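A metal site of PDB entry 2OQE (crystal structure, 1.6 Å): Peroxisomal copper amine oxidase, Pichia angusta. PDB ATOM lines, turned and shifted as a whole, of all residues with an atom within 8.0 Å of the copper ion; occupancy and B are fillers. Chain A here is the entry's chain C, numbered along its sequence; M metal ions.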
ATOM      1  N   VAL A 291      -7.467  -3.577  22.206  1.00  0.00           N
ATOM      2  CA  VAL A 291      -6.250  -3.755  22.992  1.00  0.00           C
ATOM      3  C   VAL A 291      -6.527  -3.253  24.422  1.00  0.00           C
ATOM      4  O   VAL A 291      -6.103  -2.142  24.803  1.00  0.00           O
ATOM      5  CB  VAL A 291      -5.054  -3.017  22.341  1.00  0.00           C
ATOM      6  CG1 VAL A 291      -3.778  -3.247  23.149  1.00  0.00           C
ATOM      7  CG2 VAL A 291      -4.871  -3.520  20.899  1.00  0.00           C
ATOM      8  N   TYR A 293      -6.384  -2.533  28.254  1.00  0.00           N
ATOM      9  CA  TYR A 293      -5.422  -2.494  29.350  1.00  0.00           C
ATOM     10  C   TYR A 293      -6.070  -2.911  30.645  1.00  0.00           C
ATOM     11  O   TYR A 293      -7.310  -2.804  30.818  1.00  0.00           O
ATOM     12  CB  TYR A 293      -4.775  -1.098  29.448  1.00  0.00           C
ATOM     13  CG  TYR A 293      -3.673  -0.974  28.459  1.00  0.00           C
ATOM     14  CD1 TYR A 293      -2.339  -1.059  28.848  1.00  0.00           C
ATOM     15  CD2 TYR A 293      -3.953  -0.883  27.088  1.00  0.00           C
ATOM     16  CE1 TYR A 293      -1.331  -0.996  27.911  1.00  0.00           C
ATOM     17  CE2 TYR A 293      -2.954  -0.815  26.149  1.00  0.00           C
ATOM     18  CZ  TYR A 293      -1.650  -0.875  26.556  1.00  0.00           C
ATOM     19  OH  TYR A 293      -0.671  -0.832  25.597  1.00  0.00           O
ATOM     20  N   ASN A 392       2.678   3.721  19.554  1.00  0.00           N
ATOM     21  CA  ASN A 392       3.809   2.963  20.088  1.00  0.00           C
ATOM     22  C   ASN A 392       3.965   1.565  19.494  1.00  0.00           C
ATOM     23  O   ASN A 392       5.104   1.067  19.447  1.00  0.00           O
ATOM     24  CB  ASN A 392       3.724   2.869  21.627  1.00  0.00           C
ATOM     25  CG  ASN A 392       2.403   2.297  22.096  1.00  0.00           C
ATOM     26  OD1 ASN A 392       1.351   2.907  21.912  1.00  0.00           O
ATOM     27  ND2 ASN A 392       2.451   1.117  22.676  1.00  0.00           N
ATOM     28  N   TPQ A 393       2.902   0.989  19.042  1.00  0.00           N
ATOM     29  CA  TPQ A 393       2.729  -0.407  18.624  1.00  0.00           C
ATOM     30  CB  TPQ A 393       1.290  -0.961  18.743  1.00  0.00           C
ATOM     31  C   TPQ A 393       3.135  -0.559  17.178  1.00  0.00           C
ATOM     32  O   TPQ A 393       2.526   0.208  16.401  1.00  0.00           O
ATOM     33  C1  TPQ A 393       0.526  -0.747  20.037  1.00  0.00           C
ATOM     34  C2  TPQ A 393       0.999  -1.357  21.322  1.00  0.00           C
ATOM     35  O2  TPQ A 393       2.131  -2.116  21.364  1.00  0.00           O
ATOM     36  C3  TPQ A 393       0.279  -1.169  22.501  1.00  0.00           C
ATOM     37  C4  TPQ A 393      -0.876  -0.396  22.473  1.00  0.00           C
ATOM     38  O4  TPQ A 393      -1.613  -0.178  23.585  1.00  0.00           O
ATOM     39  C5  TPQ A 393      -1.372   0.198  21.223  1.00  0.00           C
ATOM     40  O5  TPQ A 393      -2.537   0.907  21.309  1.00  0.00           O
ATOM     41  C6  TPQ A 393      -0.654   0.016  20.028  1.00  0.00           C
ATOM     42  N   TYR A 395       2.311  -3.612  14.267  1.00  0.00           N
ATOM     43  CA  TYR A 395       1.678  -4.887  13.946  1.00  0.00           C
ATOM     44  C   TYR A 395       2.123  -5.291  12.548  1.00  0.00           C
ATOM     45  O   TYR A 395       1.833  -4.568  11.586  1.00  0.00           O
ATOM     46  CB  TYR A 395       0.155  -4.737  13.969  1.00  0.00           C
ATOM     47  CG  TYR A 395      -0.398  -4.445  15.345  1.00  0.00           C
ATOM     48  CD1 TYR A 395      -0.712  -5.474  16.219  1.00  0.00           C
ATOM     49  CD2 TYR A 395      -0.589  -3.140  15.797  1.00  0.00           C
ATOM     50  CE1 TYR A 395      -1.211  -5.218  17.498  1.00  0.00           C
ATOM     51  CE2 TYR A 395      -1.082  -2.878  17.073  1.00  0.00           C
ATOM     52  CZ  TYR A 395      -1.396  -3.928  17.913  1.00  0.00           C
ATOM     53  OH  TYR A 395      -1.886  -3.683  19.188  1.00  0.00           O
ATOM     54  N   LEU A 413       3.989  -8.833  16.701  1.00  0.00           N
ATOM     55  CA  LEU A 413       3.801  -7.584  17.431  1.00  0.00           C
ATOM     56  C   LEU A 413       5.175  -7.121  17.828  1.00  0.00           C
ATOM     57  O   LEU A 413       5.913  -7.877  18.455  1.00  0.00           O
ATOM     58  CB  LEU A 413       2.997  -7.807  18.727  1.00  0.00           C
ATOM     59  CG  LEU A 413       1.631  -8.492  18.742  1.00  0.00           C
ATOM     60  CD1 LEU A 413       0.968  -8.390  20.111  1.00  0.00           C
ATOM     61  CD2 LEU A 413       0.735  -7.889  17.700  1.00  0.00           C
ATOM     62  N   THR A 414       5.479  -5.880  17.510  1.00  0.00           N
ATOM     63  CA  THR A 414       6.725  -5.279  17.970  1.00  0.00           C
ATOM     64  C   THR A 414       6.450  -3.812  18.290  1.00  0.00           C
ATOM     65  O   THR A 414       5.311  -3.469  18.596  1.00  0.00           O
ATOM     66  CB  THR A 414       7.916  -5.551  16.969  1.00  0.00           C
ATOM     67  OG1 THR A 414       9.116  -4.969  17.454  1.00  0.00           O
ATOM     68  CG2 THR A 414       7.624  -5.040  15.547  1.00  0.00           C
ATOM     69  N   ILE A 416       6.897  -0.493  20.819  1.00  0.00           N
ATOM     70  CA  ILE A 416       7.242  -0.074  22.175  1.00  0.00           C
ATOM     71  C   ILE A 416       6.038  -0.233  23.090  1.00  0.00           C
ATOM     72  O   ILE A 416       4.907   0.037  22.688  1.00  0.00           O
ATOM     73  CB  ILE A 416       7.758   1.383  22.171  1.00  0.00           C
ATOM     74  CG1 ILE A 416       8.950   1.483  21.198  1.00  0.00           C
ATOM     75  CG2 ILE A 416       8.187   1.805  23.598  1.00  0.00           C
ATOM     76  CD1 ILE A 416       9.397   2.858  20.936  1.00  0.00           C
ATOM     77  N   LEU A 417       6.306  -0.688  24.318  1.00  0.00           N
ATOM     78  CA  LEU A 417       5.277  -0.740  25.355  1.00  0.00           C
ATOM     79  C   LEU A 417       4.660   0.620  25.601  1.00  0.00           C
ATOM     80  O   LEU A 417       5.374   1.628  25.692  1.00  0.00           O
ATOM     81  CB  LEU A 417       5.912  -1.207  26.666  1.00  0.00           C
ATOM     82  CG  LEU A 417       6.465  -2.633  26.728  1.00  0.00           C
ATOM     83  CD1 LEU A 417       7.257  -2.846  28.026  1.00  0.00           C
ATOM     84  CD2 LEU A 417       5.304  -3.631  26.628  1.00  0.00           C
ATOM     85  N   ASN A 418       3.346   0.646  25.779  1.00  0.00           N
ATOM     86  CA  ASN A 418       2.732   1.837  26.377  1.00  0.00           C
ATOM     87  C   ASN A 418       3.181   1.882  27.839  1.00  0.00           C
ATOM     88  O   ASN A 418       3.129   0.877  28.555  1.00  0.00           O
ATOM     89  CB  ASN A 418       1.218   1.794  26.277  1.00  0.00           C
ATOM     90  CG  ASN A 418       0.556   2.774  27.231  1.00  0.00           C
ATOM     91  OD1 ASN A 418       0.244   2.418  28.366  1.00  0.00           O
ATOM     92  ND2 ASN A 418       0.357   4.003  26.797  1.00  0.00           N
ATOM     93  N   HIS A 442       1.687  -1.274  31.848  1.00  0.00           N
ATOM     94  CA  HIS A 442       0.459  -1.898  32.315  1.00  0.00           C
ATOM     95  C   HIS A 442       0.151  -3.171  31.527  1.00  0.00           C
ATOM     96  O   HIS A 442       0.491  -3.259  30.338  1.00  0.00           O
ATOM     97  CB  HIS A 442      -0.728  -0.938  32.127  1.00  0.00           C
ATOM     98  CG  HIS A 442      -0.733   0.212  33.080  1.00  0.00           C
ATOM     99  ND1 HIS A 442      -1.248   1.448  32.735  1.00  0.00           N
ATOM    100  CD2 HIS A 442      -0.298   0.337  34.356  1.00  0.00           C
ATOM    101  CE1 HIS A 442      -1.145   2.272  33.761  1.00  0.00           C
ATOM    102  NE2 HIS A 442      -0.563   1.628  34.757  1.00  0.00           N
ATOM    103  N   ASN A 443      -0.506  -4.128  32.194  1.00  0.00           N
ATOM    104  CA  ASN A 443      -0.969  -5.364  31.572  1.00  0.00           C
ATOM    105  C   ASN A 443      -1.979  -4.996  30.493  1.00  0.00           C
ATOM    106  O   ASN A 443      -2.739  -4.049  30.664  1.00  0.00           O
ATOM    107  CB  ASN A 443      -1.693  -6.231  32.600  1.00  0.00           C
ATOM    108  CG  ASN A 443      -0.792  -6.640  33.766  1.00  0.00           C
ATOM    109  OD1 ASN A 443       0.452  -6.585  33.665  1.00  0.00           O
ATOM    110  ND2 ASN A 443      -1.408  -7.047  34.873  1.00  0.00           N
ATOM    111  N   HIS A 444      -2.033  -5.782  29.431  1.00  0.00           N
ATOM    112  CA  HIS A 444      -3.067  -5.566  28.404  1.00  0.00           C
ATOM    113  C   HIS A 444      -3.206  -6.808  27.548  1.00  0.00           C
ATOM    114  O   HIS A 444      -2.322  -7.662  27.544  1.00  0.00           O
ATOM    115  CB  HIS A 444      -2.691  -4.366  27.537  1.00  0.00           C
ATOM    116  CG  HIS A 444      -1.328  -4.494  26.934  1.00  0.00           C
ATOM    117  ND1 HIS A 444      -0.170  -4.328  27.671  1.00  0.00           N
ATOM    118  CD2 HIS A 444      -0.926  -4.815  25.673  1.00  0.00           C
ATOM    119  CE1 HIS A 444       0.875  -4.546  26.897  1.00  0.00           C
ATOM    120  NE2 HIS A 444       0.445  -4.829  25.678  1.00  0.00           N
ATOM    121  N   GLN A 445      -4.306  -6.878  26.807  1.00  0.00           N
ATOM    122  CA  GLN A 445      -4.511  -7.932  25.813  1.00  0.00           C
ATOM    123  C   GLN A 445      -4.465  -7.306  24.426  1.00  0.00           C
ATOM    124  O   GLN A 445      -4.769  -6.124  24.274  1.00  0.00           O
ATOM    125  CB  GLN A 445      -5.888  -8.590  25.990  1.00  0.00           C
ATOM    126  CG  GLN A 445      -6.062  -9.226  27.373  1.00  0.00           C
ATOM    127  CD  GLN A 445      -7.310 -10.055  27.436  1.00  0.00           C
ATOM    128  OE1 GLN A 445      -8.418  -9.516  27.587  1.00  0.00           O
ATOM    129  NE2 GLN A 445      -7.153 -11.388  27.301  1.00  0.00           N
ATOM    130  N   HIS A 446      -4.062  -8.092  23.425  1.00  0.00           N
ATOM    131  CA  HIS A 446      -4.241  -7.660  22.032  1.00  0.00           C
ATOM    132  C   HIS A 446      -5.225  -8.645  21.421  1.00  0.00           C
ATOM    133  O   HIS A 446      -4.900  -9.833  21.299  1.00  0.00           O
ATOM    134  CB  HIS A 446      -2.938  -7.731  21.235  1.00  0.00           C
ATOM    135  CG  HIS A 446      -1.808  -6.910  21.789  1.00  0.00           C
ATOM    136  ND1 HIS A 446      -1.477  -5.676  21.271  1.00  0.00           N
ATOM    137  CD2 HIS A 446      -0.887  -7.186  22.734  1.00  0.00           C
ATOM    138  CE1 HIS A 446      -0.420  -5.206  21.913  1.00  0.00           C
ATOM    139  NE2 HIS A 446      -0.020  -6.115  22.784  1.00  0.00           N
ATOM    140  N   ILE A 610      -3.483 -12.290  22.184  1.00  0.00           N
ATOM    141  CA  ILE A 610      -2.608 -12.659  23.287  1.00  0.00           C
ATOM    142  C   ILE A 610      -2.904 -11.785  24.493  1.00  0.00           C
ATOM    143  O   ILE A 610      -3.518 -10.722  24.383  1.00  0.00           O
ATOM    144  CB  ILE A 610      -1.107 -12.497  22.924  1.00  0.00           C
ATOM    145  CG1 ILE A 610      -0.773 -11.046  22.538  1.00  0.00           C
ATOM    146  CG2 ILE A 610      -0.695 -13.517  21.827  1.00  0.00           C
ATOM    147  CD1 ILE A 610       0.699 -10.669  22.777  1.00  0.00           C
ATOM    148  N   THR A 611      -2.413 -12.254  25.636  1.00  0.00           N
ATOM    149  CA  THR A 611      -2.471 -11.482  26.864  1.00  0.00           C
ATOM    150  C   THR A 611      -1.025 -11.160  27.210  1.00  0.00           C
ATOM    151  O   THR A 611      -0.172 -12.056  27.283  1.00  0.00           O
ATOM    152  CB  THR A 611      -3.137 -12.304  27.970  1.00  0.00           C
ATOM    153  OG1 THR A 611      -4.478 -12.651  27.569  1.00  0.00           O
ATOM    154  CG2 THR A 611      -3.206 -11.519  29.273  1.00  0.00           C
ATOM    155  N   HIS A 612      -0.757  -9.871  27.388  1.00  0.00           N
ATOM    156  CA  HIS A 612       0.619  -9.370  27.532  1.00  0.00           C
ATOM    157  C   HIS A 612       0.883  -8.883  28.975  1.00  0.00           C
ATOM    158  O   HIS A 612       0.278  -7.902  29.424  1.00  0.00           O
ATOM    159  CB  HIS A 612       0.870  -8.240  26.506  1.00  0.00           C
ATOM    160  CG  HIS A 612       2.298  -7.827  26.360  1.00  0.00           C
ATOM    161  ND1 HIS A 612       2.735  -6.988  25.361  1.00  0.00           N
ATOM    162  CD2 HIS A 612       3.407  -8.146  27.083  1.00  0.00           C
ATOM    163  CE1 HIS A 612       4.036  -6.793  25.480  1.00  0.00           C
ATOM    164  NE2 HIS A 612       4.463  -7.477  26.525  1.00  0.00           N
ATOM    165  N   PHE A 613       1.765  -9.588  29.688  1.00  0.00           N
ATOM    166  CA  PHE A 613       2.251  -9.136  30.988  1.00  0.00           C
ATOM    167  C   PHE A 613       3.689  -8.690  30.772  1.00  0.00           C
ATOM    168  O   PHE A 613       4.588  -9.532  30.628  1.00  0.00           O
ATOM    169  CB  PHE A 613       2.165 -10.251  32.052  1.00  0.00           C
ATOM    170  CG  PHE A 613       0.769 -10.711  32.326  1.00  0.00           C
ATOM    171  CD1 PHE A 613      -0.082  -9.967  33.123  1.00  0.00           C
ATOM    172  CD2 PHE A 613       0.297 -11.897  31.766  1.00  0.00           C
ATOM    173  CE1 PHE A 613      -1.417 -10.387  33.334  1.00  0.00           C
ATOM    174  CE2 PHE A 613      -1.017 -12.345  32.008  1.00  0.00           C
ATOM    175  CZ  PHE A 613      -1.864 -11.588  32.785  1.00  0.00           C
ATOM    176  N   PRO A 614       3.907  -7.358  30.681  1.00  0.00           N
ATOM    177  CA  PRO A 614       5.232  -6.880  30.275  1.00  0.00           C
ATOM    178  C   PRO A 614       6.354  -7.337  31.186  1.00  0.00           C
ATOM    179  O   PRO A 614       6.151  -7.569  32.383  1.00  0.00           O
ATOM    180  CB  PRO A 614       5.092  -5.351  30.351  1.00  0.00           C
ATOM    181  CG  PRO A 614       3.622  -5.132  30.100  1.00  0.00           C
ATOM    182  CD  PRO A 614       2.961  -6.256  30.867  1.00  0.00           C
ATOM    183  N   ASP A 618      11.008  -6.694  27.172  1.00  0.00           N
ATOM    184  CA  ASP A 618      10.141  -6.007  26.182  1.00  0.00           C
ATOM    185  C   ASP A 618      10.526  -4.561  25.968  1.00  0.00           C
ATOM    186  O   ASP A 618       9.936  -3.876  25.113  1.00  0.00           O
ATOM    187  CB  ASP A 618       8.694  -6.004  26.688  1.00  0.00           C
ATOM    188  CG  ASP A 618       8.084  -7.389  26.788  1.00  0.00           C
ATOM    189  OD1 ASP A 618       8.555  -8.322  26.102  1.00  0.00           O
ATOM    190  OD2 ASP A 618       7.101  -7.525  27.557  1.00  0.00           O
ATOM    191  N   MET A 622      10.419  -3.745  21.847  1.00  0.00           N
ATOM    192  CA  MET A 622       9.992  -5.128  22.079  1.00  0.00           C
ATOM    193  C   MET A 622      10.377  -6.110  20.981  1.00  0.00           C
ATOM    194  O   MET A 622      10.074  -5.867  19.833  1.00  0.00           O
ATOM    195  CB  MET A 622       8.498  -5.178  22.284  1.00  0.00           C
ATOM    196  CG  MET A 622       8.088  -6.555  22.728  1.00  0.00           C
ATOM    197  SD  MET A 622       6.366  -6.575  23.175  1.00  0.00           S
ATOM    198  CE  MET A 622       5.595  -6.395  21.563  1.00  0.00           C
ATOM    199  N   GLU A 625       6.692 -10.606  18.988  1.00  0.00           N
ATOM    200  CA  GLU A 625       5.887 -11.657  19.609  1.00  0.00           C
ATOM    201  C   GLU A 625       4.939 -12.238  18.561  1.00  0.00           C
ATOM    202  O   GLU A 625       4.167 -11.487  17.950  1.00  0.00           O
ATOM    203  CB  GLU A 625       5.080 -11.106  20.776  1.00  0.00           C
ATOM    204  CG  GLU A 625       4.145 -12.151  21.392  1.00  0.00           C
ATOM    205  CD  GLU A 625       3.848 -11.939  22.871  1.00  0.00           C
ATOM    206  OE1 GLU A 625       4.173 -10.842  23.416  1.00  0.00           O
ATOM    207  OE2 GLU A 625       3.268 -12.866  23.483  1.00  0.00           O
HETATM  208 CU    CU M   1       1.367  -6.083  24.224  1.00  0.00          CU
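NE2 of His 612 lies within hydrogen-bond range of OD2 of Asp 618, at 2.8 Å. N of His 446 lies within hydrogen-bond range of O of Ile 610. A ring nitrogen (ND1) of His 446 lies within hydrogen-bond range of the side-chain hydroxyl (OH) of Tyr 395 (2.9 Å). ND1 of His 444 is in hydrogen-bond range of O of His 442 (2.9 Å).
Of the 23 residues printed, 3 come within 4 Å of the copper ion. The nearest printed residue that does not touch the copper ion is Leu 413 (4.7 Å).
The copper ion is bound by a ring nitrogen (ND1) of His 612, a ring nitrogen (NE2) of His 446 and a ring nitrogen (NE2) of His 444. The copper ion has three donor atoms within binding distance.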
